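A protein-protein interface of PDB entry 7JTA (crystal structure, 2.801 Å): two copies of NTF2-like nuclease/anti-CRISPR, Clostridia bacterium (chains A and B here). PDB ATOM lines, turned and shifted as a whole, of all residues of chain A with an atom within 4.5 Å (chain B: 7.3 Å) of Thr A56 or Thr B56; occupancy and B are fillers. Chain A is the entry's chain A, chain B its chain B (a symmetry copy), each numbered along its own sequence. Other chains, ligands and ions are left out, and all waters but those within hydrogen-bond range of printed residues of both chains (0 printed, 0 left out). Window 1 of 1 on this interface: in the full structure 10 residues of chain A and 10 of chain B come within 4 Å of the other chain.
Ile A54 touches Val B57, and with the chains exchanged Val A57 touches Ile B54. Ser A55 touches Thr B56, and with the chains exchanged Thr A56 touches Ser B55. Thr A56 touches its own counterpart, Thr B56. 7 positions are printed for both chains.
Thr A56 touches two residues of chain B. Of chain A, only Ser A55 and Thr A56 come within 4 Å of Thr B56. Printed residues of chain A within 4 Å of Pro B53: Tyr A34. Of the printed residues of chain B, Ile A54 touches Val B57 (3.6 Å) and Leu B58 (2.9 Å). Of the printed residues of chain B, Val A57 touches Ile B54 (3.7 Å). Printed residues of chain A within 4 Å of Ser B55: Thr A56. Leu B37 touches none of the printed residues of chain A. The nearest printed residue of chain A that does not touch Pro B53 is Val A57 (6.4 Å).
The backbone NH of Arg A35 sits at hydrogen-bond distance from the backbone carbonyl oxygen of Val A57, at 2.8 Å. The side-chain amide nitrogen (NE2) of Gln A36 sits at hydrogen-bond distance from the side-chain hydroxyl (OG1) of Thr A56. The side-chain amide oxygen (OE1) of Gln B36 lies within hydrogen-bond range of the side-chain hydroxyl (OG1) of Thr B56 (3.3 Å). The backbone NH (N) of Ile B54 sits at hydrogen-bond distance from the backbone carbonyl oxygen (O) of Leu B37. The backbone carbonyl oxygen (O) of Val B57 lies within hydrogen-bond range of the backbone NH (N) of Arg B35 (2.8 Å). N of Leu B37 lies within hydrogen-bond range of O of Ser B55, 2.9 Å away.
N of Leu B58 sits at hydrogen-bond distance from O of Ile A54. OH of Tyr A34 sits at hydrogen-bond distance from O of Pro B53, at 2.7 Å. The backbone carbonyl oxygen of Thr B56 lies within hydrogen-bond range of the backbone NH of Thr A56, at 2.7 Å.
Printed residues of chain B that touch a printed residue of chain A: Pro B53, Ile B54, Ser B55, Thr B56, Val B57 and Leu B58. Along chain B the printed residues that touch a printed residue of chain A span positions 53 to 58. Among the printed residues, 7 pairs touch across the chains. Among the printed residues, no Asp or Glu carboxylate lies within 4 Å of a Lys or Arg side-chain nitrogen of the other chain.
Among the printed residues, merely in contact across the chains: Ile A54 with Val B57, Ser A55 with Thr B56, Thr A56 with Ser B55 and Val A57 with Ile B54.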
ATOM      1  N   TYR A  34     -14.046  14.347  30.993  1.00  0.00           N
ATOM      2  CA  TYR A  34     -14.396  14.916  29.700  1.00  0.00           C
ATOM      3  C   TYR A  34     -13.621  14.227  28.583  1.00  0.00           C
ATOM      4  O   TYR A  34     -12.484  13.787  28.773  1.00  0.00           O
ATOM      5  CB  TYR A  34     -14.114  16.427  29.665  1.00  0.00           C
ATOM      6  CG  TYR A  34     -14.968  17.230  30.615  1.00  0.00           C
ATOM      7  CD1 TYR A  34     -14.524  17.523  31.900  1.00  0.00           C
ATOM      8  CD2 TYR A  34     -16.221  17.689  30.231  1.00  0.00           C
ATOM      9  CE1 TYR A  34     -15.305  18.256  32.773  1.00  0.00           C
ATOM     10  CE2 TYR A  34     -17.008  18.423  31.097  1.00  0.00           C
ATOM     11  CZ  TYR A  34     -16.548  18.704  32.365  1.00  0.00           C
ATOM     12  OH  TYR A  34     -17.335  19.435  33.224  1.00  0.00           O
ATOM     13  N   ARG A  35     -14.244  14.155  27.409  1.00  0.00           N
ATOM     14  CA  ARG A  35     -13.604  13.651  26.200  1.00  0.00           C
ATOM     15  C   ARG A  35     -13.409  14.809  25.229  1.00  0.00           C
ATOM     16  O   ARG A  35     -14.388  15.397  24.757  1.00  0.00           O
ATOM     17  CB  ARG A  35     -14.429  12.541  25.552  1.00  0.00           C
ATOM     18  CG  ARG A  35     -13.807  12.005  24.272  1.00  0.00           C
ATOM     19  CD  ARG A  35     -14.599  10.837  23.719  1.00  0.00           C
ATOM     20  NE  ARG A  35     -13.816  10.049  22.772  1.00  0.00           N
ATOM     21  CZ  ARG A  35     -14.068   9.979  21.468  1.00  0.00           C
ATOM     22  NH1 ARG A  35     -15.086  10.651  20.948  1.00  0.00           N
ATOM     23  NH2 ARG A  35     -13.300   9.236  20.682  1.00  0.00           N
ATOM     24  N   GLN A  36     -12.150  15.126  24.935  1.00  0.00           N
ATOM     25  CA  GLN A  36     -11.788  16.197  24.017  1.00  0.00           C
ATOM     26  C   GLN A  36     -11.246  15.623  22.715  1.00  0.00           C
ATOM     27  O   GLN A  36     -10.345  14.778  22.732  1.00  0.00           O
ATOM     28  CB  GLN A  36     -10.748  17.124  24.643  1.00  0.00           C
ATOM     29  CG  GLN A  36     -10.314  18.259  23.727  1.00  0.00           C
ATOM     30  CD  GLN A  36      -9.439  19.265  24.439  1.00  0.00           C
ATOM     31  OE1 GLN A  36      -8.212  19.203  24.364  1.00  0.00           O
ATOM     32  NE2 GLN A  36     -10.070  20.202  25.140  1.00  0.00           N
ATOM     33  N   ILE A  54     -11.343  20.807  18.977  1.00  0.00           N
ATOM     34  CA  ILE A  54     -12.557  20.798  18.181  1.00  0.00           C
ATOM     35  C   ILE A  54     -13.800  20.684  19.052  1.00  0.00           C
ATOM     36  O   ILE A  54     -14.787  21.383  18.816  1.00  0.00           O
ATOM     37  CB  ILE A  54     -12.524  19.669  17.129  1.00  0.00           C
ATOM     38  CG1 ILE A  54     -11.384  19.892  16.133  1.00  0.00           C
ATOM     39  CG2 ILE A  54     -13.868  19.568  16.418  1.00  0.00           C
ATOM     40  CD1 ILE A  54     -11.381  18.885  15.011  1.00  0.00           C
ATOM     41  N   SER A  55     -13.770  19.819  20.064  1.00  0.00           N
ATOM     42  CA  SER A  55     -14.943  19.620  20.900  1.00  0.00           C
ATOM     43  C   SER A  55     -14.536  18.940  22.198  1.00  0.00           C
ATOM     44  O   SER A  55     -13.626  18.110  22.223  1.00  0.00           O
ATOM     45  CB  SER A  55     -16.004  18.792  20.176  1.00  0.00           C
ATOM     46  OG  SER A  55     -15.690  17.416  20.229  1.00  0.00           O
ATOM     47  N   THR A  56     -15.208  19.333  23.276  1.00  0.00           N
ATOM     48  CA  THR A  56     -15.087  18.688  24.575  1.00  0.00           C
ATOM     49  C   THR A  56     -16.488  18.386  25.082  1.00  0.00           C
ATOM     50  O   THR A  56     -17.403  19.192  24.905  1.00  0.00           O
ATOM     51  CB  THR A  56     -14.340  19.560  25.576  1.00  0.00           C
ATOM     52  OG1 THR A  56     -13.095  19.988  25.004  1.00  0.00           O
ATOM     53  CG2 THR A  56     -14.063  18.775  26.852  1.00  0.00           C
ATOM     54  N   VAL A  57     -16.662  17.211  25.679  1.00  0.00           N
ATOM     55  CA  VAL A  57     -17.971  16.771  26.149  1.00  0.00           C
ATOM     56  C   VAL A  57     -17.805  16.044  27.473  1.00  0.00           C
ATOM     57  O   VAL A  57     -16.812  15.341  27.689  1.00  0.00           O
ATOM     58  CB  VAL A  57     -18.676  15.864  25.121  1.00  0.00           C
ATOM     59  CG1 VAL A  57     -20.059  15.495  25.609  1.00  0.00           C
ATOM     60  CG2 VAL A  57     -18.755  16.559  23.775  1.00  0.00           C
ATOM     61  N   ALA B  25     -21.589  30.308  26.905  1.00  0.00           N
ATOM     62  CA  ALA B  25     -20.467  31.223  26.804  1.00  0.00           C
ATOM     63  C   ALA B  25     -19.827  31.084  25.432  1.00  0.00           C
ATOM     64  O   ALA B  25     -19.808  29.999  24.850  1.00  0.00           O
ATOM     65  CB  ALA B  25     -19.429  30.969  27.899  1.00  0.00           C
ATOM     66  N   LEU B  27     -16.205  31.437  23.914  1.00  0.00           N
ATOM     67  CA  LEU B  27     -14.794  31.490  24.267  1.00  0.00           C
ATOM     68  C   LEU B  27     -13.975  31.767  23.015  1.00  0.00           C
ATOM     69  O   LEU B  27     -14.321  31.308  21.923  1.00  0.00           O
ATOM     70  CB  LEU B  27     -14.356  30.174  24.906  1.00  0.00           C
ATOM     71  CG  LEU B  27     -15.242  29.644  26.035  1.00  0.00           C
ATOM     72  CD1 LEU B  27     -14.652  28.389  26.648  1.00  0.00           C
ATOM     73  CD2 LEU B  27     -15.438  30.706  27.103  1.00  0.00           C
ATOM     74  N   ARG B  33     -13.109  30.635  17.888  1.00  0.00           N
ATOM     75  CA  ARG B  33     -14.269  30.866  18.741  1.00  0.00           C
ATOM     76  C   ARG B  33     -14.953  29.552  19.099  1.00  0.00           C
ATOM     77  O   ARG B  33     -15.160  28.687  18.241  1.00  0.00           O
ATOM     78  CB  ARG B  33     -15.278  31.804  18.070  1.00  0.00           C
ATOM     79  CG  ARG B  33     -14.798  33.237  17.942  1.00  0.00           C
ATOM     80  CD  ARG B  33     -15.964  34.203  18.009  1.00  0.00           C
ATOM     81  NE  ARG B  33     -17.065  33.763  17.160  1.00  0.00           N
ATOM     82  CZ  ARG B  33     -18.295  34.264  17.212  1.00  0.00           C
ATOM     83  NH1 ARG B  33     -18.586  35.226  18.079  1.00  0.00           N
ATOM     84  NH2 ARG B  33     -19.235  33.800  16.401  1.00  0.00           N
ATOM     85  N   TYR B  34     -15.313  29.416  20.374  1.00  0.00           N
ATOM     86  CA  TYR B  34     -15.959  28.222  20.894  1.00  0.00           C
ATOM     87  C   TYR B  34     -17.257  28.593  21.595  1.00  0.00           C
ATOM     88  O   TYR B  34     -17.391  29.682  22.161  1.00  0.00           O
ATOM     89  CB  TYR B  34     -15.051  27.477  21.879  1.00  0.00           C
ATOM     90  CG  TYR B  34     -13.813  26.904  21.246  1.00  0.00           C
ATOM     91  CD1 TYR B  34     -12.635  27.631  21.204  1.00  0.00           C
ATOM     92  CD2 TYR B  34     -13.827  25.639  20.674  1.00  0.00           C
ATOM     93  CE1 TYR B  34     -11.499  27.111  20.619  1.00  0.00           C
ATOM     94  CE2 TYR B  34     -12.701  25.112  20.091  1.00  0.00           C
ATOM     95  CZ  TYR B  34     -11.539  25.851  20.065  1.00  0.00           C
ATOM     96  OH  TYR B  34     -10.413  25.324  19.483  1.00  0.00           O
ATOM     97  N   ARG B  35     -18.209  27.668  21.557  1.00  0.00           N
ATOM     98  CA  ARG B  35     -19.470  27.787  22.277  1.00  0.00           C
ATOM     99  C   ARG B  35     -19.479  26.764  23.403  1.00  0.00           C
ATOM    100  O   ARG B  35     -19.450  25.554  23.149  1.00  0.00           O
ATOM    101  CB  ARG B  35     -20.657  27.572  21.342  1.00  0.00           C
ATOM    102  CG  ARG B  35     -22.009  27.628  22.035  1.00  0.00           C
ATOM    103  CD  ARG B  35     -23.128  27.505  21.015  1.00  0.00           C
ATOM    104  NE  ARG B  35     -24.412  27.955  21.540  1.00  0.00           N
ATOM    105  CZ  ARG B  35     -25.437  27.144  21.784  1.00  0.00           C
ATOM    106  NH1 ARG B  35     -25.320  25.843  21.552  1.00  0.00           N
ATOM    107  NH2 ARG B  35     -26.578  27.632  22.256  1.00  0.00           N
ATOM    108  N   GLN B  36     -19.506  27.250  24.639  1.00  0.00           N
ATOM    109  CA  GLN B  36     -19.536  26.404  25.823  1.00  0.00           C
ATOM    110  C   GLN B  36     -20.911  26.466  26.475  1.00  0.00           C
ATOM    111  O   GLN B  36     -21.427  27.555  26.746  1.00  0.00           O
ATOM    112  CB  GLN B  36     -18.468  26.836  26.824  1.00  0.00           C
ATOM    113  CG  GLN B  36     -18.460  26.013  28.090  1.00  0.00           C
ATOM    114  CD  GLN B  36     -17.286  26.352  28.974  1.00  0.00           C
ATOM    115  OE1 GLN B  36     -16.328  25.587  29.069  1.00  0.00           O
ATOM    116  NE2 GLN B  36     -17.350  27.507  29.626  1.00  0.00           N
ATOM    117  N   LEU B  37     -21.496  25.300  26.722  1.00  0.00           N
ATOM    118  CA  LEU B  37     -22.747  25.171  27.453  1.00  0.00           C
ATOM    119  C   LEU B  37     -22.459  24.609  28.838  1.00  0.00           C
ATOM    120  O   LEU B  37     -21.769  23.592  28.967  1.00  0.00           O
ATOM    121  CB  LEU B  37     -23.727  24.270  26.704  1.00  0.00           C
ATOM    122  CG  LEU B  37     -24.170  24.811  25.346  1.00  0.00           C
ATOM    123  CD1 LEU B  37     -24.992  23.780  24.596  1.00  0.00           C
ATOM    124  CD2 LEU B  37     -24.955  26.100  25.521  1.00  0.00           C
ATOM    125  N   SER B  38     -22.975  25.278  29.867  1.00  0.00           N
ATOM    126  CA  SER B  38     -22.796  24.854  31.248  1.00  0.00           C
ATOM    127  C   SER B  38     -24.149  24.823  31.947  1.00  0.00           C
ATOM    128  O   SER B  38     -25.138  25.377  31.461  1.00  0.00           O
ATOM    129  CB  SER B  38     -21.833  25.775  32.004  1.00  0.00           C
ATOM    130  OG  SER B  38     -20.703  26.088  31.211  1.00  0.00           O
ATOM    131  N   PRO B  53     -19.549  22.682  33.548  1.00  0.00           N
ATOM    132  CA  PRO B  53     -19.450  22.694  32.083  1.00  0.00           C
ATOM    133  C   PRO B  53     -19.899  21.365  31.492  1.00  0.00           C
ATOM    134  O   PRO B  53     -19.546  20.293  31.987  1.00  0.00           O
ATOM    135  CB  PRO B  53     -17.958  22.944  31.832  1.00  0.00           C
ATOM    136  CG  PRO B  53     -17.450  23.548  33.097  1.00  0.00           C
ATOM    137  CD  PRO B  53     -18.248  22.915  34.192  1.00  0.00           C
ATOM    138  N   ILE B  54     -20.679  21.446  30.416  1.00  0.00           N
ATOM    139  CA  ILE B  54     -21.261  20.275  29.780  1.00  0.00           C
ATOM    140  C   ILE B  54     -20.594  19.964  28.446  1.00  0.00           C
ATOM    141  O   ILE B  54     -20.309  18.802  28.151  1.00  0.00           O
ATOM    142  CB  ILE B  54     -22.784  20.448  29.602  1.00  0.00           C
ATOM    143  CG1 ILE B  54     -23.462  20.579  30.965  1.00  0.00           C
ATOM    144  CG2 ILE B  54     -23.366  19.284  28.805  1.00  0.00           C
ATOM    145  CD1 ILE B  54     -23.107  19.471  31.923  1.00  0.00           C
ATOM    146  N   SER B  55     -20.343  20.982  27.627  1.00  0.00           N
ATOM    147  CA  SER B  55     -19.778  20.746  26.309  1.00  0.00           C
ATOM    148  C   SER B  55     -19.209  22.045  25.763  1.00  0.00           C
ATOM    149  O   SER B  55     -19.771  23.119  25.983  1.00  0.00           O
ATOM    150  CB  SER B  55     -20.834  20.194  25.350  1.00  0.00           C
ATOM    151  OG  SER B  55     -21.662  21.233  24.850  1.00  0.00           O
ATOM    152  N   THR B  56     -18.096  21.933  25.047  1.00  0.00           N
ATOM    153  CA  THR B  56     -17.516  23.046  24.316  1.00  0.00           C
ATOM    154  C   THR B  56     -17.278  22.582  22.891  1.00  0.00           C
ATOM    155  O   THR B  56     -16.815  21.461  22.666  1.00  0.00           O
ATOM    156  CB  THR B  56     -16.200  23.522  24.942  1.00  0.00           C
ATOM    157  OG1 THR B  56     -16.387  23.763  26.343  1.00  0.00           O
ATOM    158  CG2 THR B  56     -15.728  24.807  24.278  1.00  0.00           C
ATOM    159  N   VAL B  57     -17.600  23.434  21.929  1.00  0.00           N
ATOM    160  CA  VAL B  57     -17.478  23.068  20.525  1.00  0.00           C
ATOM    161  C   VAL B  57     -16.962  24.269  19.752  1.00  0.00           C
ATOM    162  O   VAL B  57     -17.293  25.417  20.069  1.00  0.00           O
ATOM    163  CB  VAL B  57     -18.816  22.571  19.940  1.00  0.00           C
ATOM    164  CG1 VAL B  57     -19.745  23.747  19.674  1.00  0.00           C
ATOM    165  CG2 VAL B  57     -18.570  21.789  18.670  1.00  0.00           C
ATOM    166  N   LEU B  58     -16.143  23.999  18.742  1.00  0.00           N
ATOM    167  CA  LEU B  58     -15.657  25.039  17.850  1.00  0.00           C
ATOM    168  C   LEU B  58     -16.807  25.555  16.995  1.00  0.00           C
ATOM    169  O   LEU B  58     -17.588  24.769  16.450  1.00  0.00           O
ATOM    170  CB  LEU B  58     -14.546  24.476  16.967  1.00  0.00           C
ATOM    171  CG  LEU B  58     -13.736  25.372  16.035  1.00  0.00           C
ATOM    172  CD1 LEU B  58     -12.792  26.259  16.837  1.00  0.00           C
ATOM    173  CD2 LEU B  58     -12.967  24.512  15.041  1.00  0.00           C
